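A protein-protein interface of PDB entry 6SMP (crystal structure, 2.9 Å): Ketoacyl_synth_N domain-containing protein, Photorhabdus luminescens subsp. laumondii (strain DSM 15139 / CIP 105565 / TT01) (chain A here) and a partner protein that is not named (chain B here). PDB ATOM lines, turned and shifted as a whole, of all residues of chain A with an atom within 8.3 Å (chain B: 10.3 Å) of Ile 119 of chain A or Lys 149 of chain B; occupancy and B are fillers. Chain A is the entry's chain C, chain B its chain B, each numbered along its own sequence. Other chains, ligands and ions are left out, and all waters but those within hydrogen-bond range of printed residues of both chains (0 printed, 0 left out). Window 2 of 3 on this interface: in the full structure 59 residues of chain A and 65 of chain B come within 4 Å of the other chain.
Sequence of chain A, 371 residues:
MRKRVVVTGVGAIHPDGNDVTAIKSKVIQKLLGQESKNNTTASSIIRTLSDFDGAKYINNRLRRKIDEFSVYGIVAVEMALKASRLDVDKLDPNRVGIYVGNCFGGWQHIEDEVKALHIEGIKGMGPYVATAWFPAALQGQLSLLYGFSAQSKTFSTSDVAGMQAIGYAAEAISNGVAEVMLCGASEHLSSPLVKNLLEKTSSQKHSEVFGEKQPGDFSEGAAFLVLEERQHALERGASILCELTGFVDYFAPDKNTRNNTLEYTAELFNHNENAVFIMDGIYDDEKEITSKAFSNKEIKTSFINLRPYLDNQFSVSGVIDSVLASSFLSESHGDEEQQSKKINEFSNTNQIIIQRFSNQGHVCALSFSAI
Among the printed residues, merely in contact across the chains: Val 114 of chain A with Leu 141 of chain B (3.8 Å), Lys 115 of chain A with Thr 145 of chain B (3.9 Å), Lys 115 of chain A with Gly 148 of chain B (3.997 Å), Lys 115 of chain A with Glu 150 of chain B (3.8 Å), Leu 117 of chain A with Phe 68 of chain B (3.4 Å), Leu 117 of chain A with Pro 224 of chain B (3.5 Å), His 118 of chain A with Phe 68 of chain B (3.5 Å), His 118 of chain A with Leu 142 of chain B (2.8 Å), Ile 119 of chain A with Gly 147 of chain B (3.5 Å), Ile 119 of chain A with Gly 148 of chain B (3.9 Å), Ile 119 of chain A with Lys 149 of chain B (3.8 Å), Gly 121 of chain A with Phe 68 of chain B (3.6 Å) and Ile 122 of chain A with Gly 69 of chain B (3.5 Å).
OG1 of Thr 145 of chain B lies within hydrogen-bond range of N of Gly 148 of chain B, 3.3 Å away. O of Leu 142 of chain B sits at hydrogen-bond distance from N of Gly 147 of chain B (2.8 Å). O of Leu 141 of chain B lies within hydrogen-bond range of OG1 of Thr 145 of chain B (2.7 Å). The backbone carbonyl oxygen (O) of Thr 145 of chain B lies within hydrogen-bond range of the backbone NH (N) of Glu 150 of chain B, 3.2 Å away.
The guanidinium group of Arg 67 of chain B sits at hydrogen-bond distance from the backbone carbonyl oxygen of His 118 of chain A (3.0 Å). The backbone carbonyl oxygen of Phe 68 of chain B is in hydrogen-bond range of the backbone NH of Ile 122 of chain A (3.1 Å). The side-chain carboxylate of Glu 138 of chain B is in hydrogen-bond range of a ring nitrogen (NE2) of His 118 of chain A, 3.4 Å away.
Of the 20 printed residues of chain B, 12 touch a printed residue of chain A. Printed residues of chain B that touch a printed residue of chain A: Arg 67, Phe 68, Gly 69, Glu 138, Leu 141, Leu 142, Thr 145, Gly 147, Gly 148, Lys 149, Glu 150 and Pro 224. Hydrophobic or aromatic side chains of chain B that line the printed part of chain A: Phe 68, Leu 141, Leu 142 and Pro 224. Of the 12 printed residues of chain A, 7 touch a printed residue of chain B. Printed residues of chain A that touch a printed residue of chain B: Val 114, Lys 115, Leu 117, His 118, Ile 119, Gly 121 and Ile 122. Among the printed residues, 16 pairs touch across the chains. Among the printed residues, no Asp or Glu carboxylate lies within 4 Å of a Lys or Arg side-chain nitrogen of the other chain.
Of the printed residues of chain B, Val 114 of chain A touches Leu 141. No residue of chain B comes within 4 Å of Ala 116 of chain A. Printed residues of chain B within 4 Å of Leu 117 of chain A: Phe 68 (3.4 Å) and Pro 224 (3.5 Å). Of chain B, only Gly 147, Gly 148 and Lys 149 come within 4 Å of Ile 119 of chain A. No residue of chain B comes within 4 Å of Glu 120 of chain A. Printed residues of chain A within 4 Å of Leu 141 of chain B: Val 114 (3.8 Å). Ile 144 of chain B touches none of the printed residues of chain A. Ile 152 of chain B touches none of the printed residues of chain A. Printed residues of chain A within 4 Å of Pro 224 of chain B: Leu 117 (3.5 Å). The nearest residue of chain A that does not touch Lys 149 of chain B is Lys 115 of chain A (5.6 Å). The nearest printed residue of chain A that does not touch Glu 150 of chain B is Ile 119 of chain A (7.3 Å).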
ATOM      1  N   ASP A 112       1.602 -16.395   2.014  1.00  0.00           N
ATOM      2  CA  ASP A 112       2.613 -15.690   2.793  1.00  0.00           C
ATOM      3  C   ASP A 112       3.795 -16.603   3.116  1.00  0.00           C
ATOM      4  O   ASP A 112       4.916 -16.122   3.273  1.00  0.00           O
ATOM      5  CB  ASP A 112       2.016 -15.072   4.061  1.00  0.00           C
ATOM      6  CG  ASP A 112       1.023 -13.953   3.791  1.00  0.00           C
ATOM      7  OD1 ASP A 112       1.309 -13.110   2.916  1.00  0.00           O
ATOM      8  OD2 ASP A 112      -0.030 -13.934   4.459  1.00  0.00           O
ATOM      9  N   GLU A 113       3.534 -17.912   3.213  1.00  0.00           N
ATOM     10  CA  GLU A 113       4.557 -18.898   3.529  1.00  0.00           C
ATOM     11  C   GLU A 113       5.423 -19.178   2.301  1.00  0.00           C
ATOM     12  O   GLU A 113       6.602 -19.500   2.442  1.00  0.00           O
ATOM     13  CB  GLU A 113       3.923 -20.186   4.060  1.00  0.00           C
ATOM     14  CG  GLU A 113       3.133 -20.000   5.344  1.00  0.00           C
ATOM     15  CD  GLU A 113       2.601 -21.290   5.944  1.00  0.00           C
ATOM     16  OE1 GLU A 113       3.423 -22.149   6.318  1.00  0.00           O
ATOM     17  OE2 GLU A 113       1.366 -21.435   6.029  1.00  0.00           O
ATOM     18  N   VAL A 114       4.829 -19.058   1.104  1.00  0.00           N
ATOM     19  CA  VAL A 114       5.538 -19.262  -0.152  1.00  0.00           C
ATOM     20  C   VAL A 114       6.544 -18.127  -0.343  1.00  0.00           C
ATOM     21  O   VAL A 114       7.673 -18.362  -0.774  1.00  0.00           O
ATOM     22  CB  VAL A 114       4.576 -19.371  -1.355  1.00  0.00           C
ATOM     23  CG1 VAL A 114       5.321 -19.508  -2.676  1.00  0.00           C
ATOM     24  CG2 VAL A 114       3.579 -20.507  -1.189  1.00  0.00           C
ATOM     25  N   LYS A 115       6.115 -16.903  -0.014  1.00  0.00           N
ATOM     26  CA  LYS A 115       6.961 -15.723  -0.098  1.00  0.00           C
ATOM     27  C   LYS A 115       8.020 -15.772   1.000  1.00  0.00           C
ATOM     28  O   LYS A 115       9.164 -15.381   0.774  1.00  0.00           O
ATOM     29  CB  LYS A 115       6.125 -14.443   0.013  1.00  0.00           C
ATOM     30  CG  LYS A 115       5.137 -14.204  -1.121  1.00  0.00           C
ATOM     31  CD  LYS A 115       4.643 -12.773  -1.207  1.00  0.00           C
ATOM     32  CE  LYS A 115       3.817 -12.343  -0.013  1.00  0.00           C
ATOM     33  NZ  LYS A 115       3.300 -10.964  -0.172  1.00  0.00           N
ATOM     34  N   ALA A 116       7.625 -16.266   2.181  1.00  0.00           N
ATOM     35  CA  ALA A 116       8.498 -16.324   3.344  1.00  0.00           C
ATOM     36  C   ALA A 116       9.620 -17.342   3.139  1.00  0.00           C
ATOM     37  O   ALA A 116      10.686 -17.207   3.738  1.00  0.00           O
ATOM     38  CB  ALA A 116       7.697 -16.633   4.585  1.00  0.00           C
ATOM     39  N   LEU A 117       9.354 -18.367   2.344  1.00  0.00           N
ATOM     40  CA  LEU A 117      10.352 -19.444   2.146  1.00  0.00           C
ATOM     41  C   LEU A 117      11.543 -18.893   1.379  1.00  0.00           C
ATOM     42  O   LEU A 117      12.606 -19.465   1.472  1.00  0.00           O
ATOM     43  CB  LEU A 117       9.684 -20.608   1.409  1.00  0.00           C
ATOM     44  CG  LEU A 117      10.605 -21.533   0.615  1.00  0.00           C
ATOM     45  CD1 LEU A 117      11.228 -22.586   1.495  1.00  0.00           C
ATOM     46  CD2 LEU A 117       9.853 -22.198  -0.511  1.00  0.00           C
ATOM     47  N   HIS A 118      11.369 -17.773   0.701  1.00  0.00           N
ATOM     48  CA  HIS A 118      12.488 -17.231  -0.107  1.00  0.00           C
ATOM     49  C   HIS A 118      13.367 -16.276   0.704  1.00  0.00           C
ATOM     50  O   HIS A 118      14.579 -16.303   0.516  1.00  0.00           O
ATOM     51  CB  HIS A 118      11.927 -16.603  -1.379  1.00  0.00           C
ATOM     52  CG  HIS A 118      11.631 -17.613  -2.431  1.00  0.00           C
ATOM     53  ND1 HIS A 118      12.544 -17.960  -3.392  1.00  0.00           N
ATOM     54  CD2 HIS A 118      10.536 -18.361  -2.663  1.00  0.00           C
ATOM     55  CE1 HIS A 118      12.025 -18.870  -4.175  1.00  0.00           C
ATOM     56  NE2 HIS A 118      10.799 -19.135  -3.747  1.00  0.00           N
ATOM     57  N   ILE A 119      12.760 -15.529   1.619  1.00  0.00           N
ATOM     58  CA  ILE A 119      13.404 -14.507   2.433  1.00  0.00           C
ATOM     59  C   ILE A 119      14.003 -15.133   3.693  1.00  0.00           C
ATOM     60  O   ILE A 119      15.121 -14.790   4.075  1.00  0.00           O
ATOM     61  CB  ILE A 119      12.469 -13.310   2.730  1.00  0.00           C
ATOM     62  CG1 ILE A 119      11.315 -13.681   3.668  1.00  0.00           C
ATOM     63  CG2 ILE A 119      11.975 -12.674   1.437  1.00  0.00           C
ATOM     64  CD1 ILE A 119      10.385 -12.536   4.005  1.00  0.00           C
ATOM     65  N   GLU A 120      13.265 -16.057   4.327  1.00  0.00           N
ATOM     66  CA  GLU A 120      13.690 -16.675   5.575  1.00  0.00           C
ATOM     67  C   GLU A 120      14.437 -17.976   5.291  1.00  0.00           C
ATOM     68  O   GLU A 120      15.597 -18.126   5.670  1.00  0.00           O
ATOM     69  CB  GLU A 120      12.490 -16.978   6.479  1.00  0.00           C
ATOM     70  CG  GLU A 120      11.772 -15.751   7.011  1.00  0.00           C
ATOM     71  CD  GLU A 120      10.684 -16.056   8.030  1.00  0.00           C
ATOM     72  OE1 GLU A 120       9.541 -15.604   7.823  1.00  0.00           O
ATOM     73  OE2 GLU A 120      10.985 -16.740   9.030  1.00  0.00           O
ATOM     74  N   GLY A 121      13.745 -18.910   4.628  1.00  0.00           N
ATOM     75  CA  GLY A 121      14.209 -20.277   4.444  1.00  0.00           C
ATOM     76  C   GLY A 121      13.097 -21.275   4.763  1.00  0.00           C
ATOM     77  O   GLY A 121      11.919 -20.942   4.657  1.00  0.00           O
ATOM     78  N   ILE A 122      13.488 -22.488   5.177  1.00  0.00           N
ATOM     79  CA  ILE A 122      12.550 -23.547   5.525  1.00  0.00           C
ATOM     80  C   ILE A 122      11.658 -23.118   6.693  1.00  0.00           C
ATOM     81  O   ILE A 122      10.497 -23.518   6.757  1.00  0.00           O
ATOM     82  CB  ILE A 122      13.279 -24.882   5.800  1.00  0.00           C
ATOM     83  CG1 ILE A 122      12.291 -26.039   5.987  1.00  0.00           C
ATOM     84  CG2 ILE A 122      14.251 -24.759   6.968  1.00  0.00           C
ATOM     85  CD1 ILE A 122      12.941 -27.391   6.169  1.00  0.00           C
ATOM     86  N   GLY A 124      10.218 -20.468   7.401  1.00  0.00           N
ATOM     87  CA  GLY A 124       9.078 -19.652   7.008  1.00  0.00           C
ATOM     88  C   GLY A 124       7.830 -20.488   6.730  1.00  0.00           C
ATOM     89  O   GLY A 124       6.711 -20.014   6.921  1.00  0.00           O
ATOM     90  N   GLU B  66      21.637 -25.369   0.134  1.00  0.00           N
ATOM     91  CA  GLU B  66      22.364 -24.108   0.176  1.00  0.00           C
ATOM     92  C   GLU B  66      21.402 -22.930   0.322  1.00  0.00           C
ATOM     93  O   GLU B  66      21.509 -22.156   1.273  1.00  0.00           O
ATOM     94  CB  GLU B  66      23.230 -23.935  -1.074  1.00  0.00           C
ATOM     95  CG  GLU B  66      24.381 -24.920  -1.178  1.00  0.00           C
ATOM     96  CD  GLU B  66      25.189 -24.811  -2.461  1.00  0.00           C
ATOM     97  OE1 GLU B  66      25.710 -25.847  -2.919  1.00  0.00           O
ATOM     98  OE2 GLU B  66      25.300 -23.689  -3.000  1.00  0.00           O
ATOM     99  N   ARG B  67      20.470 -22.803  -0.632  1.00  0.00           N
ATOM    100  CA  ARG B  67      19.638 -21.618  -0.779  1.00  0.00           C
ATOM    101  C   ARG B  67      18.540 -21.586   0.286  1.00  0.00           C
ATOM    102  O   ARG B  67      18.336 -20.552   0.922  1.00  0.00           O
ATOM    103  CB  ARG B  67      19.095 -21.517  -2.212  1.00  0.00           C
ATOM    104  CG  ARG B  67      17.992 -20.487  -2.422  1.00  0.00           C
ATOM    105  CD  ARG B  67      18.351 -19.038  -2.146  1.00  0.00           C
ATOM    106  NE  ARG B  67      17.182 -18.175  -2.280  1.00  0.00           N
ATOM    107  CZ  ARG B  67      17.138 -16.887  -1.952  1.00  0.00           C
ATOM    108  NH1 ARG B  67      16.019 -16.204  -2.120  1.00  0.00           N
ATOM    109  NH2 ARG B  67      18.206 -16.286  -1.457  1.00  0.00           N
ATOM    110  N   PHE B  68      17.797 -22.686   0.443  1.00  0.00           N
ATOM    111  CA  PHE B  68      16.586 -22.709   1.315  1.00  0.00           C
ATOM    112  C   PHE B  68      16.801 -23.422   2.648  1.00  0.00           C
ATOM    113  O   PHE B  68      15.929 -23.356   3.507  1.00  0.00           O
ATOM    114  CB  PHE B  68      15.402 -23.313   0.564  1.00  0.00           C
ATOM    115  CG  PHE B  68      15.052 -22.591  -0.706  1.00  0.00           C
ATOM    116  CD1 PHE B  68      15.554 -23.011  -1.915  1.00  0.00           C
ATOM    117  CD2 PHE B  68      14.241 -21.476  -0.685  1.00  0.00           C
ATOM    118  CE1 PHE B  68      15.233 -22.336  -3.075  1.00  0.00           C
ATOM    119  CE2 PHE B  68      13.929 -20.796  -1.844  1.00  0.00           C
ATOM    120  CZ  PHE B  68      14.432 -21.227  -3.036  1.00  0.00           C
ATOM    121  N   GLY B  69      17.917 -24.114   2.787  1.00  0.00           N
ATOM    122  CA  GLY B  69      18.242 -24.757   4.049  1.00  0.00           C
ATOM    123  C   GLY B  69      17.412 -26.016   4.293  1.00  0.00           C
ATOM    124  O   GLY B  69      17.040 -26.301   5.430  1.00  0.00           O
ATOM    125  N   LEU B  90      15.135 -19.036 -10.274  1.00  0.00           N
ATOM    126  CA  LEU B  90      13.799 -19.576 -10.629  1.00  0.00           C
ATOM    127  C   LEU B  90      13.591 -19.402 -12.130  1.00  0.00           C
ATOM    128  O   LEU B  90      13.957 -18.349 -12.635  1.00  0.00           O
ATOM    129  CB  LEU B  90      12.744 -18.729  -9.916  1.00  0.00           C
ATOM    130  CG  LEU B  90      12.364 -19.118  -8.490  1.00  0.00           C
ATOM    131  CD1 LEU B  90      11.121 -18.367  -8.053  1.00  0.00           C
ATOM    132  CD2 LEU B  90      12.150 -20.611  -8.361  1.00  0.00           C
ATOM    133  N   GLU B 138       4.525 -20.455  -8.711  1.00  0.00           N
ATOM    134  CA  GLU B 138       5.422 -19.913  -7.667  1.00  0.00           C
ATOM    135  C   GLU B 138       6.374 -18.880  -8.273  1.00  0.00           C
ATOM    136  O   GLU B 138       6.723 -17.945  -7.578  1.00  0.00           O
ATOM    137  CB  GLU B 138       6.157 -21.077  -7.023  1.00  0.00           C
ATOM    138  CG  GLU B 138       7.192 -20.667  -6.018  1.00  0.00           C
ATOM    139  CD  GLU B 138       8.350 -21.626  -6.068  1.00  0.00           C
ATOM    140  OE1 GLU B 138       8.516 -22.259  -7.094  1.00  0.00           O
ATOM    141  OE2 GLU B 138       9.064 -21.728  -5.094  1.00  0.00           O
ATOM    142  N   LEU B 141       4.392 -15.544  -8.570  1.00  0.00           N
ATOM    143  CA  LEU B 141       4.148 -14.881  -7.296  1.00  0.00           C
ATOM    144  C   LEU B 141       5.385 -14.103  -6.844  1.00  0.00           C
ATOM    145  O   LEU B 141       5.262 -12.971  -6.380  1.00  0.00           O
ATOM    146  CB  LEU B 141       3.716 -15.927  -6.258  1.00  0.00           C
ATOM    147  CG  LEU B 141       3.542 -15.447  -4.815  1.00  0.00           C
ATOM    148  CD1 LEU B 141       2.466 -14.376  -4.705  1.00  0.00           C
ATOM    149  CD2 LEU B 141       3.215 -16.614  -3.895  1.00  0.00           C
ATOM    150  N   LEU B 142       6.569 -14.707  -6.998  1.00  0.00           N
ATOM    151  CA  LEU B 142       7.805 -14.143  -6.473  1.00  0.00           C
ATOM    152  C   LEU B 142       8.364 -13.065  -7.403  1.00  0.00           C
ATOM    153  O   LEU B 142       9.097 -12.186  -6.953  1.00  0.00           O
ATOM    154  CB  LEU B 142       8.819 -15.268  -6.243  1.00  0.00           C
ATOM    155  CG  LEU B 142       8.421 -16.288  -5.179  1.00  0.00           C
ATOM    156  CD1 LEU B 142       9.144 -17.605  -5.392  1.00  0.00           C
ATOM    157  CD2 LEU B 142       8.674 -15.755  -3.776  1.00  0.00           C
ATOM    158  N   ARG B 143       8.015 -13.145  -8.693  1.00  0.00           N
ATOM    159  CA  ARG B 143       8.436 -12.165  -9.684  1.00  0.00           C
ATOM    160  C   ARG B 143       7.713 -10.840  -9.443  1.00  0.00           C
ATOM    161  O   ARG B 143       8.349  -9.787  -9.409  1.00  0.00           O
ATOM    162  CB  ARG B 143       8.160 -12.693 -11.096  1.00  0.00           C
ATOM    163  CG  ARG B 143       8.680 -11.813 -12.225  1.00  0.00           C
ATOM    164  CD  ARG B 143       7.741 -11.834 -13.418  1.00  0.00           C
ATOM    165  NE  ARG B 143       7.358 -13.184 -13.813  1.00  0.00           N
ATOM    166  CZ  ARG B 143       6.322 -13.492 -14.588  1.00  0.00           C
ATOM    167  NH1 ARG B 143       6.072 -14.757 -14.878  1.00  0.00           N
ATOM    168  NH2 ARG B 143       5.539 -12.543 -15.068  1.00  0.00           N
ATOM    169  N   ILE B 144       6.385 -10.907  -9.270  1.00  0.00           N
ATOM    170  CA  ILE B 144       5.541  -9.723  -9.163  1.00  0.00           C
ATOM    171  C   ILE B 144       5.712  -9.053  -7.798  1.00  0.00           C
ATOM    172  O   ILE B 144       5.419  -7.867  -7.660  1.00  0.00           O
ATOM    173  CB  ILE B 144       4.061 -10.035  -9.488  1.00  0.00           C
ATOM    174  CG1 ILE B 144       3.420 -10.966  -8.452  1.00  0.00           C
ATOM    175  CG2 ILE B 144       3.921 -10.566 -10.908  1.00  0.00           C
ATOM    176  CD1 ILE B 144       2.021 -11.431  -8.797  1.00  0.00           C
ATOM    177  N   THR B 145       6.184  -9.810  -6.798  1.00  0.00           N
ATOM    178  CA  THR B 145       6.386  -9.287  -5.452  1.00  0.00           C
ATOM    179  C   THR B 145       7.855  -8.930  -5.214  1.00  0.00           C
ATOM    180  O   THR B 145       8.203  -8.459  -4.132  1.00  0.00           O
ATOM    181  CB  THR B 145       5.909 -10.265  -4.368  1.00  0.00           C
ATOM    182  OG1 THR B 145       6.580 -11.512  -4.546  1.00  0.00           O
ATOM    183  CG2 THR B 145       4.411 -10.474  -4.363  1.00  0.00           C
ATOM    184  N   LYS B 146       8.704  -9.170  -6.223  1.00  0.00           N
ATOM    185  CA  LYS B 146      10.129  -8.865  -6.180  1.00  0.00           C
ATOM    186  C   LYS B 146      10.808  -9.637  -5.050  1.00  0.00           C
ATOM    187  O   LYS B 146      11.275  -9.047  -4.077  1.00  0.00           O
ATOM    188  CB  LYS B 146      10.372  -7.353  -6.100  1.00  0.00           C
ATOM    189  CG  LYS B 146       9.981  -6.570  -7.346  1.00  0.00           C
ATOM    190  CD  LYS B 146      10.099  -5.071  -7.184  1.00  0.00           C
ATOM    191  CE  LYS B 146       9.705  -4.323  -8.439  1.00  0.00           C
ATOM    192  NZ  LYS B 146       9.794  -2.855  -8.259  1.00  0.00           N
ATOM    193  N   GLY B 147      10.852 -10.966  -5.202  1.00  0.00           N
ATOM    194  CA  GLY B 147      11.538 -11.847  -4.269  1.00  0.00           C
ATOM    195  C   GLY B 147      10.776 -12.027  -2.958  1.00  0.00           C
ATOM    196  O   GLY B 147      11.361 -12.424  -1.953  1.00  0.00           O
ATOM    197  N   GLY B 148       9.470 -11.731  -2.986  1.00  0.00           N
ATOM    198  CA  GLY B 148       8.595 -11.902  -1.835  1.00  0.00           C
ATOM    199  C   GLY B 148       8.833 -10.848  -0.755  1.00  0.00           C
ATOM    200  O   GLY B 148       8.549 -11.088   0.418  1.00  0.00           O
ATOM    201  N   LYS B 149       9.340  -9.680  -1.169  1.00  0.00           N
ATOM    202  CA  LYS B 149       9.673  -8.597  -0.256  1.00  0.00           C
ATOM    203  C   LYS B 149       8.467  -7.677  -0.078  1.00  0.00           C
ATOM    204  O   LYS B 149       8.091  -7.356   1.047  1.00  0.00           O
ATOM    205  CB  LYS B 149      10.868  -7.791  -0.781  1.00  0.00           C
ATOM    206  CG  LYS B 149      12.160  -8.570  -0.987  1.00  0.00           C
ATOM    207  CD  LYS B 149      12.839  -8.986   0.298  1.00  0.00           C
ATOM    208  CE  LYS B 149      14.126  -9.745   0.057  1.00  0.00           C
ATOM    209  NZ  LYS B 149      14.789 -10.115   1.329  1.00  0.00           N
ATOM    210  N   GLU B 150       7.874  -7.264  -1.207  1.00  0.00           N
ATOM    211  CA  GLU B 150       6.836  -6.244  -1.239  1.00  0.00           C
ATOM    212  C   GLU B 150       5.481  -6.885  -1.537  1.00  0.00           C
ATOM    213  O   GLU B 150       5.373  -8.106  -1.639  1.00  0.00           O
ATOM    214  CB  GLU B 150       7.152  -5.203  -2.317  1.00  0.00           C
ATOM    215  CG  GLU B 150       8.564  -4.645  -2.264  1.00  0.00           C
ATOM    216  CD  GLU B 150       8.871  -3.615  -3.338  1.00  0.00           C
ATOM    217  OE1 GLU B 150       8.043  -2.703  -3.538  1.00  0.00           O
ATOM    218  OE2 GLU B 150       9.935  -3.730  -3.978  1.00  0.00           O
ATOM    219  N   ASN B 151       4.453  -6.034  -1.677  1.00  0.00           N
ATOM    220  CA  ASN B 151       3.127  -6.435  -2.125  1.00  0.00           C
ATOM    221  C   ASN B 151       3.158  -6.705  -3.629  1.00  0.00           C
ATOM    222  O   ASN B 151       4.148  -6.404  -4.296  1.00  0.00           O
ATOM    223  CB  ASN B 151       2.073  -5.372  -1.798  1.00  0.00           C
ATOM    224  CG  ASN B 151       1.802  -5.215  -0.317  1.00  0.00           C
ATOM    225  OD1 ASN B 151       2.589  -5.652   0.521  1.00  0.00           O
ATOM    226  ND2 ASN B 151       0.688  -4.584   0.018  1.00  0.00           N
ATOM    227  N   ILE B 152       2.058  -7.264  -4.153  1.00  0.00           N
ATOM    228  CA  ILE B 152       1.934  -7.612  -5.561  1.00  0.00           C
ATOM    229  C   ILE B 152       1.822  -6.342  -6.403  1.00  0.00           C
ATOM    230  O   ILE B 152       1.137  -5.393  -6.024  1.00  0.00           O
ATOM    231  CB  ILE B 152       0.742  -8.567  -5.792  1.00  0.00           C
ATOM    232  CG1 ILE B 152       1.033  -9.959  -5.225  1.00  0.00           C
ATOM    233  CG2 ILE B 152       0.359  -8.629  -7.265  1.00  0.00           C
ATOM    234  CD1 ILE B 152      -0.175 -10.853  -5.113  1.00  0.00           C
ATOM    235  N   HIS B 153       2.512  -6.354  -7.551  1.00  0.00           N
ATOM    236  CA  HIS B 153       2.408  -5.320  -8.566  1.00  0.00           C
ATOM    237  C   HIS B 153       1.535  -5.829  -9.711  1.00  0.00           C
ATOM    238  O   HIS B 153       1.942  -6.734 -10.437  1.00  0.00           O
ATOM    239  CB  HIS B 153       3.802  -4.939  -9.082  1.00  0.00           C
ATOM    240  CG  HIS B 153       4.685  -4.310  -8.058  1.00  0.00           C
ATOM    241  ND1 HIS B 153       5.447  -5.054  -7.177  1.00  0.00           N
ATOM    242  CD2 HIS B 153       4.941  -3.014  -7.777  1.00  0.00           C
ATOM    243  CE1 HIS B 153       6.129  -4.244  -6.394  1.00  0.00           C
ATOM    244  NE2 HIS B 153       5.835  -2.986  -6.742  1.00  0.00           N
ATOM    245  N   PRO B 224      11.067 -25.307  -5.083  1.00  0.00           N
ATOM    246  CA  PRO B 224      11.015 -24.981  -3.657  1.00  0.00           C
ATOM    247  C   PRO B 224       9.630 -24.991  -2.998  1.00  0.00           C
ATOM    248  O   PRO B 224       9.533 -25.388  -1.888  1.00  0.00           O
ATOM    249  CB  PRO B 224      11.551 -23.553  -3.649  1.00  0.00           C
ATOM    250  CG  PRO B 224      12.543 -23.549  -4.758  1.00  0.00           C
ATOM    251  CD  PRO B 224      11.870 -24.357  -5.838  1.00  0.00           C
